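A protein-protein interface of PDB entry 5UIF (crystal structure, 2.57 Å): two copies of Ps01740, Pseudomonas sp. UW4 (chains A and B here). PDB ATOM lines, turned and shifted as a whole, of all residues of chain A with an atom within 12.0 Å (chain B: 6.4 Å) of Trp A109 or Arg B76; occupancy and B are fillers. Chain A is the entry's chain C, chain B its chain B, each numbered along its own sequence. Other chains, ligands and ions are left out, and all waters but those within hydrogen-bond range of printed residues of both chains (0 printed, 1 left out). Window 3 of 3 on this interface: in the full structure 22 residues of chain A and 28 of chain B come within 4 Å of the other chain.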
ATOM      1  N   PRO A   1     -30.344   7.537   3.144  1.00  0.00           N
ATOM      2  CA  PRO A   1     -30.825   6.804   4.320  1.00  0.00           C
ATOM      3  C   PRO A   1     -31.533   5.505   3.951  1.00  0.00           C
ATOM      4  O   PRO A   1     -32.173   5.426   2.903  1.00  0.00           O
ATOM      5  CB  PRO A   1     -31.799   7.788   4.966  1.00  0.00           C
ATOM      6  CG  PRO A   1     -32.286   8.616   3.832  1.00  0.00           C
ATOM      7  CD  PRO A   1     -31.100   8.782   2.927  1.00  0.00           C
ATOM      8  N   LEU A   2     -31.422   4.501   4.816  1.00  0.00           N
ATOM      9  CA  LEU A   2     -32.029   3.200   4.564  1.00  0.00           C
ATOM     10  C   LEU A   2     -32.824   2.711   5.770  1.00  0.00           C
ATOM     11  O   LEU A   2     -32.278   2.556   6.860  1.00  0.00           O
ATOM     12  CB  LEU A   2     -30.954   2.175   4.198  1.00  0.00           C
ATOM     13  CG  LEU A   2     -31.433   0.733   4.020  1.00  0.00           C
ATOM     14  CD1 LEU A   2     -32.386   0.624   2.839  1.00  0.00           C
ATOM     15  CD2 LEU A   2     -30.251  -0.210   3.855  1.00  0.00           C
ATOM     16  N   ARG A  64     -35.301  -0.738  11.500  1.00  0.00           N
ATOM     17  CA  ARG A  64     -33.956  -0.195  11.641  1.00  0.00           C
ATOM     18  C   ARG A  64     -33.652   0.823  10.549  1.00  0.00           C
ATOM     19  O   ARG A  64     -33.926   0.587   9.372  1.00  0.00           O
ATOM     20  CB  ARG A  64     -32.921  -1.323  11.616  1.00  0.00           C
ATOM     21  CG  ARG A  64     -31.499  -0.860  11.342  1.00  0.00           C
ATOM     22  CD  ARG A  64     -30.478  -1.892  11.792  1.00  0.00           C
ATOM     23  NE  ARG A  64     -29.169  -1.292  12.030  1.00  0.00           N
ATOM     24  CZ  ARG A  64     -28.060  -1.634  11.382  1.00  0.00           C
ATOM     25  NH1 ARG A  64     -28.096  -2.580  10.454  1.00  0.00           N
ATOM     26  NH2 ARG A  64     -26.914  -1.032  11.665  1.00  0.00           N
ATOM     27  N   GLN A  66     -30.629   3.407   8.909  1.00  0.00           N
ATOM     28  CA  GLN A  66     -29.262   3.900   8.812  1.00  0.00           C
ATOM     29  C   GLN A  66     -29.246   5.307   8.229  1.00  0.00           C
ATOM     30  O   GLN A  66     -29.630   5.516   7.079  1.00  0.00           O
ATOM     31  CB  GLN A  66     -28.401   2.964   7.961  1.00  0.00           C
ATOM     32  CG  GLN A  66     -28.016   1.668   8.655  1.00  0.00           C
ATOM     33  CD  GLN A  66     -27.083   0.815   7.819  1.00  0.00           C
ATOM     34  OE1 GLN A  66     -27.283   0.651   6.616  1.00  0.00           O
ATOM     35  NE2 GLN A  66     -26.050   0.272   8.455  1.00  0.00           N
ATOM     36  N   ILE A  67     -28.812   6.272   9.033  1.00  0.00           N
ATOM     37  CA  ILE A  67     -28.731   7.656   8.585  1.00  0.00           C
ATOM     38  C   ILE A  67     -27.299   8.165   8.680  1.00  0.00           C
ATOM     39  O   ILE A  67     -26.426   7.491   9.224  1.00  0.00           O
ATOM     40  CB  ILE A  67     -29.652   8.579   9.406  1.00  0.00           C
ATOM     41  CG1 ILE A  67     -29.133   8.721  10.838  1.00  0.00           C
ATOM     42  CG2 ILE A  67     -31.080   8.056   9.395  1.00  0.00           C
ATOM     43  CD1 ILE A  67     -29.820   9.815  11.626  1.00  0.00           C
ATOM     44  N   ARG A  68     -27.066   9.361   8.149  1.00  0.00           N
ATOM     45  CA  ARG A  68     -25.726   9.935   8.125  1.00  0.00           C
ATOM     46  C   ARG A  68     -25.386  10.615   9.445  1.00  0.00           C
ATOM     47  O   ARG A  68     -26.208  11.335  10.013  1.00  0.00           O
ATOM     48  CB  ARG A  68     -25.598  10.931   6.971  1.00  0.00           C
ATOM     49  CG  ARG A  68     -24.411  10.680   6.060  1.00  0.00           C
ATOM     50  CD  ARG A  68     -24.808  10.870   4.606  1.00  0.00           C
ATOM     51  NE  ARG A  68     -25.018  12.275   4.275  1.00  0.00           N
ATOM     52  CZ  ARG A  68     -25.611  12.702   3.165  1.00  0.00           C
ATOM     53  NH1 ARG A  68     -26.069  11.832   2.274  1.00  0.00           N
ATOM     54  NH2 ARG A  68     -25.756  14.002   2.951  1.00  0.00           N
ATOM     55  N   ALA A  69     -24.171  10.381   9.930  1.00  0.00           N
ATOM     56  CA  ALA A  69     -23.700  11.002  11.162  1.00  0.00           C
ATOM     57  C   ALA A  69     -23.557  12.509  10.980  1.00  0.00           C
ATOM     58  O   ALA A  69     -23.452  12.996   9.857  1.00  0.00           O
ATOM     59  CB  ALA A  69     -22.375  10.390  11.595  1.00  0.00           C
ATOM     60  N   GLY A  70     -23.552  13.244  12.086  1.00  0.00           N
ATOM     61  CA  GLY A  70     -23.446  14.689  12.034  1.00  0.00           C
ATOM     62  C   GLY A  70     -24.756  15.335  12.437  1.00  0.00           C
ATOM     63  O   GLY A  70     -25.006  16.503  12.143  1.00  0.00           O
ATOM     64  N   VAL A 103     -29.306   4.179  13.541  1.00  0.00           N
ATOM     65  CA  VAL A 103     -27.864   4.250  13.744  1.00  0.00           C
ATOM     66  C   VAL A 103     -27.194   5.225  12.782  1.00  0.00           C
ATOM     67  O   VAL A 103     -27.738   5.544  11.724  1.00  0.00           O
ATOM     68  CB  VAL A 103     -27.202   2.867  13.590  1.00  0.00           C
ATOM     69  CG1 VAL A 103     -27.758   1.896  14.622  1.00  0.00           C
ATOM     70  CG2 VAL A 103     -27.408   2.333  12.182  1.00  0.00           C
ATOM     71  N   ASP A 104     -26.011   5.697  13.163  1.00  0.00           N
ATOM     72  CA  ASP A 104     -25.248   6.624  12.336  1.00  0.00           C
ATOM     73  C   ASP A 104     -24.249   5.910  11.441  1.00  0.00           C
ATOM     74  O   ASP A 104     -23.548   4.994  11.869  1.00  0.00           O
ATOM     75  CB  ASP A 104     -24.506   7.642  13.202  1.00  0.00           C
ATOM     76  CG  ASP A 104     -25.365   8.826  13.567  1.00  0.00           C
ATOM     77  OD1 ASP A 104     -26.407   9.033  12.909  1.00  0.00           O
ATOM     78  OD2 ASP A 104     -24.995   9.559  14.507  1.00  0.00           O
ATOM     79  N   ILE A 105     -24.194   6.347  10.189  1.00  0.00           N
ATOM     80  CA  ILE A 105     -23.168   5.901   9.265  1.00  0.00           C
ATOM     81  C   ILE A 105     -22.401   7.113   8.759  1.00  0.00           C
ATOM     82  O   ILE A 105     -22.986   7.995   8.128  1.00  0.00           O
ATOM     83  CB  ILE A 105     -23.760   5.129   8.075  1.00  0.00           C
ATOM     84  CG1 ILE A 105     -24.533   3.902   8.564  1.00  0.00           C
ATOM     85  CG2 ILE A 105     -22.658   4.720   7.108  1.00  0.00           C
ATOM     86  CD1 ILE A 105     -23.690   2.917   9.343  1.00  0.00           C
ATOM     87  N   PRO A 106     -21.094   7.173   9.056  1.00  0.00           N
ATOM     88  CA  PRO A 106     -20.228   8.246   8.556  1.00  0.00           C
ATOM     89  C   PRO A 106     -20.363   8.407   7.046  1.00  0.00           C
ATOM     90  O   PRO A 106     -20.386   7.406   6.329  1.00  0.00           O
ATOM     91  CB  PRO A 106     -18.826   7.770   8.939  1.00  0.00           C
ATOM     92  CG  PRO A 106     -19.045   6.932  10.150  1.00  0.00           C
ATOM     93  CD  PRO A 106     -20.366   6.243   9.937  1.00  0.00           C
ATOM     94  N   ALA A 107     -20.465   9.649   6.580  1.00  0.00           N
ATOM     95  CA  ALA A 107     -20.670   9.928   5.161  1.00  0.00           C
ATOM     96  C   ALA A 107     -19.535   9.368   4.311  1.00  0.00           C
ATOM     97  O   ALA A 107     -19.720   9.061   3.133  1.00  0.00           O
ATOM     98  CB  ALA A 107     -20.812  11.426   4.933  1.00  0.00           C
ATOM     99  N   SER A 108     -18.362   9.226   4.920  1.00  0.00           N
ATOM    100  CA  SER A 108     -17.191   8.699   4.232  1.00  0.00           C
ATOM    101  C   SER A 108     -17.259   7.182   4.067  1.00  0.00           C
ATOM    102  O   SER A 108     -16.408   6.585   3.407  1.00  0.00           O
ATOM    103  CB  SER A 108     -15.919   9.083   4.989  1.00  0.00           C
ATOM    104  OG  SER A 108     -15.766  10.490   5.049  1.00  0.00           O
ATOM    105  N   TRP A 109     -18.271   6.563   4.668  1.00  0.00           N
ATOM    106  CA  TRP A 109     -18.413   5.111   4.620  1.00  0.00           C
ATOM    107  C   TRP A 109     -19.464   4.671   3.607  1.00  0.00           C
ATOM    108  O   TRP A 109     -19.667   3.476   3.391  1.00  0.00           O
ATOM    109  CB  TRP A 109     -18.773   4.557   6.002  1.00  0.00           C
ATOM    110  CG  TRP A 109     -17.696   4.717   7.034  1.00  0.00           C
ATOM    111  CD1 TRP A 109     -16.551   5.452   6.924  1.00  0.00           C
ATOM    112  CD2 TRP A 109     -17.662   4.117   8.335  1.00  0.00           C
ATOM    113  NE1 TRP A 109     -15.810   5.352   8.076  1.00  0.00           N
ATOM    114  CE2 TRP A 109     -16.470   4.537   8.957  1.00  0.00           C
ATOM    115  CE3 TRP A 109     -18.525   3.269   9.034  1.00  0.00           C
ATOM    116  CZ2 TRP A 109     -16.120   4.136  10.245  1.00  0.00           C
ATOM    117  CZ3 TRP A 109     -18.176   2.871  10.312  1.00  0.00           C
ATOM    118  CH2 TRP A 109     -16.983   3.306  10.904  1.00  0.00           C
ATOM    119  N   ALA A 110     -20.134   5.637   2.987  1.00  0.00           N
ATOM    120  CA  ALA A 110     -21.199   5.327   2.042  1.00  0.00           C
ATOM    121  C   ALA A 110     -20.964   5.981   0.686  1.00  0.00           C
ATOM    122  O   ALA A 110     -20.357   7.047   0.591  1.00  0.00           O
ATOM    123  CB  ALA A 110     -22.545   5.758   2.606  1.00  0.00           C
ATOM    124  N   MET A 111     -21.450   5.323  -0.362  1.00  0.00           N
ATOM    125  CA  MET A 111     -21.396   5.869  -1.710  1.00  0.00           C
ATOM    126  C   MET A 111     -22.726   5.638  -2.415  1.00  0.00           C
ATOM    127  O   MET A 111     -23.192   4.503  -2.528  1.00  0.00           O
ATOM    128  CB  MET A 111     -20.253   5.243  -2.506  1.00  0.00           C
ATOM    129  CG  MET A 111     -20.129   5.772  -3.922  1.00  0.00           C
ATOM    130  SD  MET A 111     -18.617   5.215  -4.723  1.00  0.00           S
ATOM    131  CE  MET A 111     -17.382   5.969  -3.666  1.00  0.00           C
ATOM    132  N   GLU A 112     -23.337   6.722  -2.879  1.00  0.00           N
ATOM    133  CA  GLU A 112     -24.670   6.661  -3.464  1.00  0.00           C
ATOM    134  C   GLU A 112     -24.680   7.219  -4.883  1.00  0.00           C
ATOM    135  O   GLU A 112     -25.216   8.298  -5.133  1.00  0.00           O
ATOM    136  CB  GLU A 112     -25.664   7.425  -2.586  1.00  0.00           C
ATOM    137  CG  GLU A 112     -25.363   7.330  -1.096  1.00  0.00           C
ATOM    138  CD  GLU A 112     -26.276   8.195  -0.252  1.00  0.00           C
ATOM    139  OE1 GLU A 112     -25.777   8.834   0.698  1.00  0.00           O
ATOM    140  OE2 GLU A 112     -27.493   8.230  -0.530  1.00  0.00           O
ATOM    141  N   GLU B  31      -7.266  -4.742  -1.834  1.00  0.00           N
ATOM    142  CA  GLU B  31      -7.086  -3.490  -1.105  1.00  0.00           C
ATOM    143  C   GLU B  31      -6.713  -3.685   0.364  1.00  0.00           C
ATOM    144  O   GLU B  31      -6.117  -2.799   0.977  1.00  0.00           O
ATOM    145  CB  GLU B  31      -8.358  -2.643  -1.199  1.00  0.00           C
ATOM    146  CG  GLU B  31      -8.687  -2.160  -2.605  1.00  0.00           C
ATOM    147  CD  GLU B  31      -7.595  -1.286  -3.200  1.00  0.00           C
ATOM    148  OE1 GLU B  31      -6.877  -0.613  -2.430  1.00  0.00           O
ATOM    149  OE2 GLU B  31      -7.454  -1.275  -4.440  1.00  0.00           O
ATOM    150  N   ILE B  67     -16.419  -4.688   7.390  1.00  0.00           N
ATOM    151  CA  ILE B  67     -14.998  -5.014   7.452  1.00  0.00           C
ATOM    152  C   ILE B  67     -14.433  -4.716   8.835  1.00  0.00           C
ATOM    153  O   ILE B  67     -15.130  -4.178   9.692  1.00  0.00           O
ATOM    154  CB  ILE B  67     -14.196  -4.233   6.397  1.00  0.00           C
ATOM    155  CG1 ILE B  67     -14.139  -2.747   6.758  1.00  0.00           C
ATOM    156  CG2 ILE B  67     -14.805  -4.428   5.019  1.00  0.00           C
ATOM    157  CD1 ILE B  67     -13.263  -1.930   5.831  1.00  0.00           C
ATOM    158  N   ARG B  71      -8.228   0.198   9.454  1.00  0.00           N
ATOM    159  CA  ARG B  71      -7.785   0.512   8.100  1.00  0.00           C
ATOM    160  C   ARG B  71      -8.134   1.948   7.708  1.00  0.00           C
ATOM    161  O   ARG B  71      -9.188   2.460   8.078  1.00  0.00           O
ATOM    162  CB  ARG B  71      -8.390  -0.477   7.098  1.00  0.00           C
ATOM    163  CG  ARG B  71      -8.333  -1.920   7.561  1.00  0.00           C
ATOM    164  CD  ARG B  71      -8.228  -2.882   6.388  1.00  0.00           C
ATOM    165  NE  ARG B  71      -7.498  -4.091   6.759  1.00  0.00           N
ATOM    166  CZ  ARG B  71      -8.054  -5.293   6.880  1.00  0.00           C
ATOM    167  NH1 ARG B  71      -9.352  -5.450   6.655  1.00  0.00           N
ATOM    168  NH2 ARG B  71      -7.316  -6.340   7.228  1.00  0.00           N
ATOM    169  N   PRO B  72      -7.236   2.602   6.954  1.00  0.00           N
ATOM    170  CA  PRO B  72      -7.406   3.999   6.541  1.00  0.00           C
ATOM    171  C   PRO B  72      -8.563   4.196   5.567  1.00  0.00           C
ATOM    172  O   PRO B  72      -9.066   3.227   4.998  1.00  0.00           O
ATOM    173  CB  PRO B  72      -6.072   4.322   5.866  1.00  0.00           C
ATOM    174  CG  PRO B  72      -5.601   3.010   5.362  1.00  0.00           C
ATOM    175  CD  PRO B  72      -5.994   2.023   6.416  1.00  0.00           C
ATOM    176  N   GLN B  73      -8.970   5.448   5.376  1.00  0.00           N
ATOM    177  CA  GLN B  73     -10.106   5.770   4.519  1.00  0.00           C
ATOM    178  C   GLN B  73      -9.864   5.425   3.051  1.00  0.00           C
ATOM    179  O   GLN B  73     -10.756   4.903   2.379  1.00  0.00           O
ATOM    180  CB  GLN B  73     -10.458   7.255   4.645  1.00  0.00           C
ATOM    181  CG  GLN B  73     -11.294   7.807   3.492  1.00  0.00           C
ATOM    182  CD  GLN B  73     -12.744   7.347   3.510  1.00  0.00           C
ATOM    183  OE1 GLN B  73     -13.083   6.307   4.080  1.00  0.00           O
ATOM    184  NE2 GLN B  73     -13.610   8.121   2.869  1.00  0.00           N
ATOM    185  N   ALA B  74      -8.662   5.721   2.564  1.00  0.00           N
ATOM    186  CA  ALA B  74      -8.313   5.492   1.162  1.00  0.00           C
ATOM    187  C   ALA B  74      -8.574   4.050   0.739  1.00  0.00           C
ATOM    188  O   ALA B  74      -8.960   3.789  -0.401  1.00  0.00           O
ATOM    189  CB  ALA B  74      -6.860   5.858   0.917  1.00  0.00           C
ATOM    190  N   THR B  75      -8.362   3.121   1.664  1.00  0.00           N
ATOM    191  CA  THR B  75      -8.646   1.713   1.416  1.00  0.00           C
ATOM    192  C   THR B  75     -10.143   1.487   1.236  1.00  0.00           C
ATOM    193  O   THR B  75     -10.574   0.857   0.269  1.00  0.00           O
ATOM    194  CB  THR B  75      -8.132   0.823   2.563  1.00  0.00           C
ATOM    195  OG1 THR B  75      -6.722   1.018   2.729  1.00  0.00           O
ATOM    196  CG2 THR B  75      -8.405  -0.643   2.265  1.00  0.00           C
ATOM    197  N   ARG B  76     -10.931   2.009   2.171  1.00  0.00           N
ATOM    198  CA  ARG B  76     -12.382   1.856   2.130  1.00  0.00           C
ATOM    199  C   ARG B  76     -12.992   2.521   0.900  1.00  0.00           C
ATOM    200  O   ARG B  76     -13.866   1.950   0.247  1.00  0.00           O
ATOM    201  CB  ARG B  76     -13.018   2.426   3.400  1.00  0.00           C
ATOM    202  CG  ARG B  76     -14.519   2.640   3.288  1.00  0.00           C
ATOM    203  CD  ARG B  76     -15.150   2.972   4.629  1.00  0.00           C
ATOM    204  NE  ARG B  76     -14.280   3.787   5.470  1.00  0.00           N
ATOM    205  CZ  ARG B  76     -13.818   3.399   6.655  1.00  0.00           C
ATOM    206  NH1 ARG B  76     -14.151   2.210   7.137  1.00  0.00           N
ATOM    207  NH2 ARG B  76     -13.032   4.201   7.359  1.00  0.00           N
ATOM    208  N   HIS B  77     -12.527   3.727   0.589  1.00  0.00           N
ATOM    209  CA  HIS B  77     -13.009   4.450  -0.582  1.00  0.00           C
ATOM    210  C   HIS B  77     -12.735   3.677  -1.866  1.00  0.00           C
ATOM    211  O   HIS B  77     -13.589   3.605  -2.751  1.00  0.00           O
ATOM    212  CB  HIS B  77     -12.365   5.832  -0.672  1.00  0.00           C
ATOM    213  CG  HIS B  77     -12.614   6.521  -1.976  1.00  0.00           C
ATOM    214  ND1 HIS B  77     -13.844   7.036  -2.324  1.00  0.00           N
ATOM    215  CD2 HIS B  77     -11.795   6.758  -3.029  1.00  0.00           C
ATOM    216  CE1 HIS B  77     -13.769   7.573  -3.529  1.00  0.00           C
ATOM    217  NE2 HIS B  77     -12.537   7.418  -3.978  1.00  0.00           N
ATOM    218  N   ALA B  78     -11.538   3.106  -1.959  1.00  0.00           N
ATOM    219  CA  ALA B  78     -11.142   2.320  -3.122  1.00  0.00           C
ATOM    220  C   ALA B  78     -12.065   1.122  -3.301  1.00  0.00           C
ATOM    221  O   ALA B  78     -12.381   0.734  -4.425  1.00  0.00           O
ATOM    222  CB  ALA B  78      -9.697   1.863  -2.989  1.00  0.00           C
ATOM    223  N   ILE B  79     -12.495   0.542  -2.186  1.00  0.00           N
ATOM    224  CA  ILE B  79     -13.441  -0.566  -2.212  1.00  0.00           C
ATOM    225  C   ILE B  79     -14.821  -0.072  -2.638  1.00  0.00           C
ATOM    226  O   ILE B  79     -15.496  -0.707  -3.448  1.00  0.00           O
ATOM    227  CB  ILE B  79     -13.541  -1.259  -0.837  1.00  0.00           C
ATOM    228  CG1 ILE B  79     -12.185  -1.843  -0.434  1.00  0.00           C
ATOM    229  CG2 ILE B  79     -14.598  -2.352  -0.860  1.00  0.00           C
ATOM    230  CD1 ILE B  79     -12.192  -2.527   0.916  1.00  0.00           C
ATOM    231  N   LEU B  80     -15.224   1.071  -2.092  1.00  0.00           N
ATOM    232  CA  LEU B  80     -16.524   1.664  -2.396  1.00  0.00           C
ATOM    233  C   LEU B  80     -16.705   1.953  -3.884  1.00  0.00           C
ATOM    234  O   LEU B  80     -17.705   1.555  -4.481  1.00  0.00           O
ATOM    235  CB  LEU B  80     -16.723   2.953  -1.594  1.00  0.00           C
ATOM    236  CG  LEU B  80     -17.080   2.812  -0.113  1.00  0.00           C
ATOM    237  CD1 LEU B  80     -16.883   4.132   0.613  1.00  0.00           C
ATOM    238  CD2 LEU B  80     -18.513   2.329   0.043  1.00  0.00           C
ATOM    239  N   ARG B  81     -15.738   2.647  -4.480  1.00  0.00           N
ATOM    240  CA  ARG B  81     -15.842   3.035  -5.883  1.00  0.00           C
ATOM    241  C   ARG B  81     -15.762   1.819  -6.801  1.00  0.00           C
ATOM    242  O   ARG B  81     -16.430   1.767  -7.833  1.00  0.00           O
ATOM    243  CB  ARG B  81     -14.748   4.039  -6.255  1.00  0.00           C
ATOM    244  CG  ARG B  81     -15.096   4.891  -7.467  1.00  0.00           C
ATOM    245  CD  ARG B  81     -16.170   5.903  -7.108  1.00  0.00           C
ATOM    246  NE  ARG B  81     -16.881   6.424  -8.271  1.00  0.00           N
ATOM    247  CZ  ARG B  81     -17.997   5.894  -8.762  1.00  0.00           C
ATOM    248  NH1 ARG B  81     -18.524   4.819  -8.195  1.00  0.00           N
ATOM    249  NH2 ARG B  81     -18.581   6.433  -9.822  1.00  0.00           N
ATOM    250  N   VAL B 100     -23.983   1.860  -1.855  1.00  0.00           N
ATOM    251  CA  VAL B 100     -22.931   1.003  -1.321  1.00  0.00           C
ATOM    252  C   VAL B 100     -22.379   1.570  -0.016  1.00  0.00           C
ATOM    253  O   VAL B 100     -22.068   2.758   0.071  1.00  0.00           O
ATOM    254  CB  VAL B 100     -21.776   0.828  -2.327  1.00  0.00           C
ATOM    255  CG1 VAL B 100     -20.734  -0.133  -1.781  1.00  0.00           C
ATOM    256  CG2 VAL B 100     -22.306   0.334  -3.664  1.00  0.00           C
ATOM    257  N   ALA B 101     -22.263   0.717   0.997  1.00  0.00           N
ATOM    258  CA  ALA B 101     -21.727   1.132   2.288  1.00  0.00           C
ATOM    259  C   ALA B 101     -20.710   0.122   2.814  1.00  0.00           C
ATOM    260  O   ALA B 101     -20.890  -1.086   2.668  1.00  0.00           O
ATOM    261  CB  ALA B 101     -22.853   1.321   3.293  1.00  0.00           C
ATOM    262  N   VAL B 102     -19.639   0.627   3.417  1.00  0.00           N
ATOM    263  CA  VAL B 102     -18.613  -0.226   4.009  1.00  0.00           C
ATOM    264  C   VAL B 102     -18.302   0.239   5.429  1.00  0.00           C
ATOM    265  O   VAL B 102     -17.616   1.240   5.628  1.00  0.00           O
ATOM    266  CB  VAL B 102     -17.318  -0.229   3.171  1.00  0.00           C
ATOM    267  CG1 VAL B 102     -16.241  -1.053   3.858  1.00  0.00           C
ATOM    268  CG2 VAL B 102     -17.587  -0.767   1.772  1.00  0.00           C
ATOM    269  N   VAL B 103     -18.815  -0.489   6.416  1.00  0.00           N
ATOM    270  CA  VAL B 103     -18.690  -0.076   7.810  1.00  0.00           C
ATOM    271  C   VAL B 103     -17.610  -0.855   8.551  1.00  0.00           C
ATOM    272  O   VAL B 103     -17.236  -1.956   8.148  1.00  0.00           O
ATOM    273  CB  VAL B 103     -20.027  -0.234   8.562  1.00  0.00           C
ATOM    274  CG1 VAL B 103     -21.094   0.648   7.934  1.00  0.00           C
ATOM    275  CG2 VAL B 103     -20.468  -1.690   8.563  1.00  0.00           C
ATOM    276  N   ASP B 104     -17.113  -0.273   9.639  1.00  0.00           N
ATOM    277  CA  ASP B 104     -16.059  -0.893  10.433  1.00  0.00           C
ATOM    278  C   ASP B 104     -16.607  -1.692  11.610  1.00  0.00           C
ATOM    279  O   ASP B 104     -17.570  -1.286  12.260  1.00  0.00           O
ATOM    280  CB  ASP B 104     -15.082   0.166  10.953  1.00  0.00           C
ATOM    281  CG  ASP B 104     -14.210   0.742   9.859  1.00  0.00           C
ATOM    282  OD1 ASP B 104     -14.012   0.058   8.833  1.00  0.00           O
ATOM    283  OD2 ASP B 104     -13.715   1.877  10.026  1.00  0.00           O
ATOM    284  N   ILE B 105     -15.981  -2.834  11.869  1.00  0.00           N
ATOM    285  CA  ILE B 105     -16.267  -3.627  13.056  1.00  0.00           C
ATOM    286  C   ILE B 105     -14.955  -4.017  13.722  1.00  0.00           C
ATOM    287  O   ILE B 105     -14.146  -4.721  13.123  1.00  0.00           O
ATOM    288  CB  ILE B 105     -17.069  -4.901  12.728  1.00  0.00           C
ATOM    289  CG1 ILE B 105     -18.436  -4.544  12.141  1.00  0.00           C
ATOM    290  CG2 ILE B 105     -17.238  -5.759  13.973  1.00  0.00           C
ATOM    291  CD1 ILE B 105     -19.299  -5.749  11.843  1.00  0.00           C
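Printed residues of chain A that touch a printed residue of chain B: Ile A105, Ser A108, Trp A109, Ala A110 and Met A111.
Of the 19 printed residues of chain B, 10 touch a printed residue of chain A.
Hydrophobic or aromatic side chains of chain B within 4 Å of the printed part of chain A: His B77, Leu B80, Val B100, Ala B101 and Val B103.
Among the printed residues, 14 pairs touch across the chains.
O of Val B100 is in hydrogen-bond range of N of Met A111, 2.7 Å away.
The backbone carbonyl oxygen (O) of Leu B80 lies close to the side-chain sulfur (SD) of Met A111, at 3.8 Å.
NH1 of Arg B81 sits close to SD of Met A111 (3.5 Å).
The backbone carbonyl oxygen (O) of Ser A108 sits at hydrogen-bond distance from the side-chain amide nitrogen (NE2) of Gln B73 (3.2 Å).
N of Val B102 is in hydrogen-bond range of O of Trp A109 (2.8 Å).
The guanidinium group of Arg B76 lies close to the indole nitrogen of Trp A109 (3.1 Å).
Of the printed residues of chain B, Ile A105 touches Val B103 (3.7 Å).
Trp A109 touches six residues of chain B.
Printed residues of chain B within 4 Å of Ala A110: Val B100.
Ile B67 touches none of the printed residues of chain A.
No residue of chain A comes within 4 Å of Pro B72.
Of the printed residues of chain A, Gln B73 touches Ser A108.
No residue of chain A comes within 4 Å of Ala B74.
No residue of chain A comes within 4 Å of Thr B75.
Of the printed residues of chain A, Arg B76 touches Trp A109 (3.1 Å).
Of chain A, only Met A111 comes within 4 Å of His B77.
No residue of chain A comes within 4 Å of Ala B78.
No residue of chain A comes within 4 Å of Ile B79.
Leu B80 touches three residues of chain A.
Printed residues of chain A within 4 Å of Ala B101: Trp A109 (3.3 Å).
Val B103 touches just these residues of chain A: Ile A105 (3.7 Å) and Trp A109 (3.6 Å).
Asp B104 touches one residue of chain A.
The nearest residue of chain B that does not touch Trp A109 is Val B100 (4.2 Å).
The nearest printed residue of chain A that does not touch Arg B76 is Ser A108 (4.02 Å).
The nearest printed residue of chain A that does not touch Val B100 is Trp A109 (4.2 Å).
O of Val B103 is in hydrogen-bond range of N of Ile B67 (3.0 Å).
N of Ile A105 lies within hydrogen-bond range of O of Ile A67 (2.7 Å).
NE of Arg B76 sits at hydrogen-bond distance from OE1 of Gln B73 (3.1 Å).
The backbone NH (N) of Ala A69 is in hydrogen-bond range of the backbone carbonyl oxygen (O) of Ile A105 (3.2 Å).
NH1 of Arg B76 is in salt-bridge range of OD1 of Asp B104 (2.7 Å).
Ile A105 touches Val B103, but with the chains exchanged Val A103 does not touch Ile B105 (11.3 Å).
Positions printed for both chains: 67, 103, 104 and 105.
Of the 14 pairs that touch across the chains among the printed residues, none has its exchanged pair printed and touching as well.
Among the printed residues, pairs that only touch across the chains: Ile A105 with Val B103, Ser A108 with Leu B80, Trp A109 with Leu B80, Trp A109 with Ala B101, Trp A109 with Val B103, Trp A109 with Asp B104, Ala A110 with Val B100 and Met A111 with His B77.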
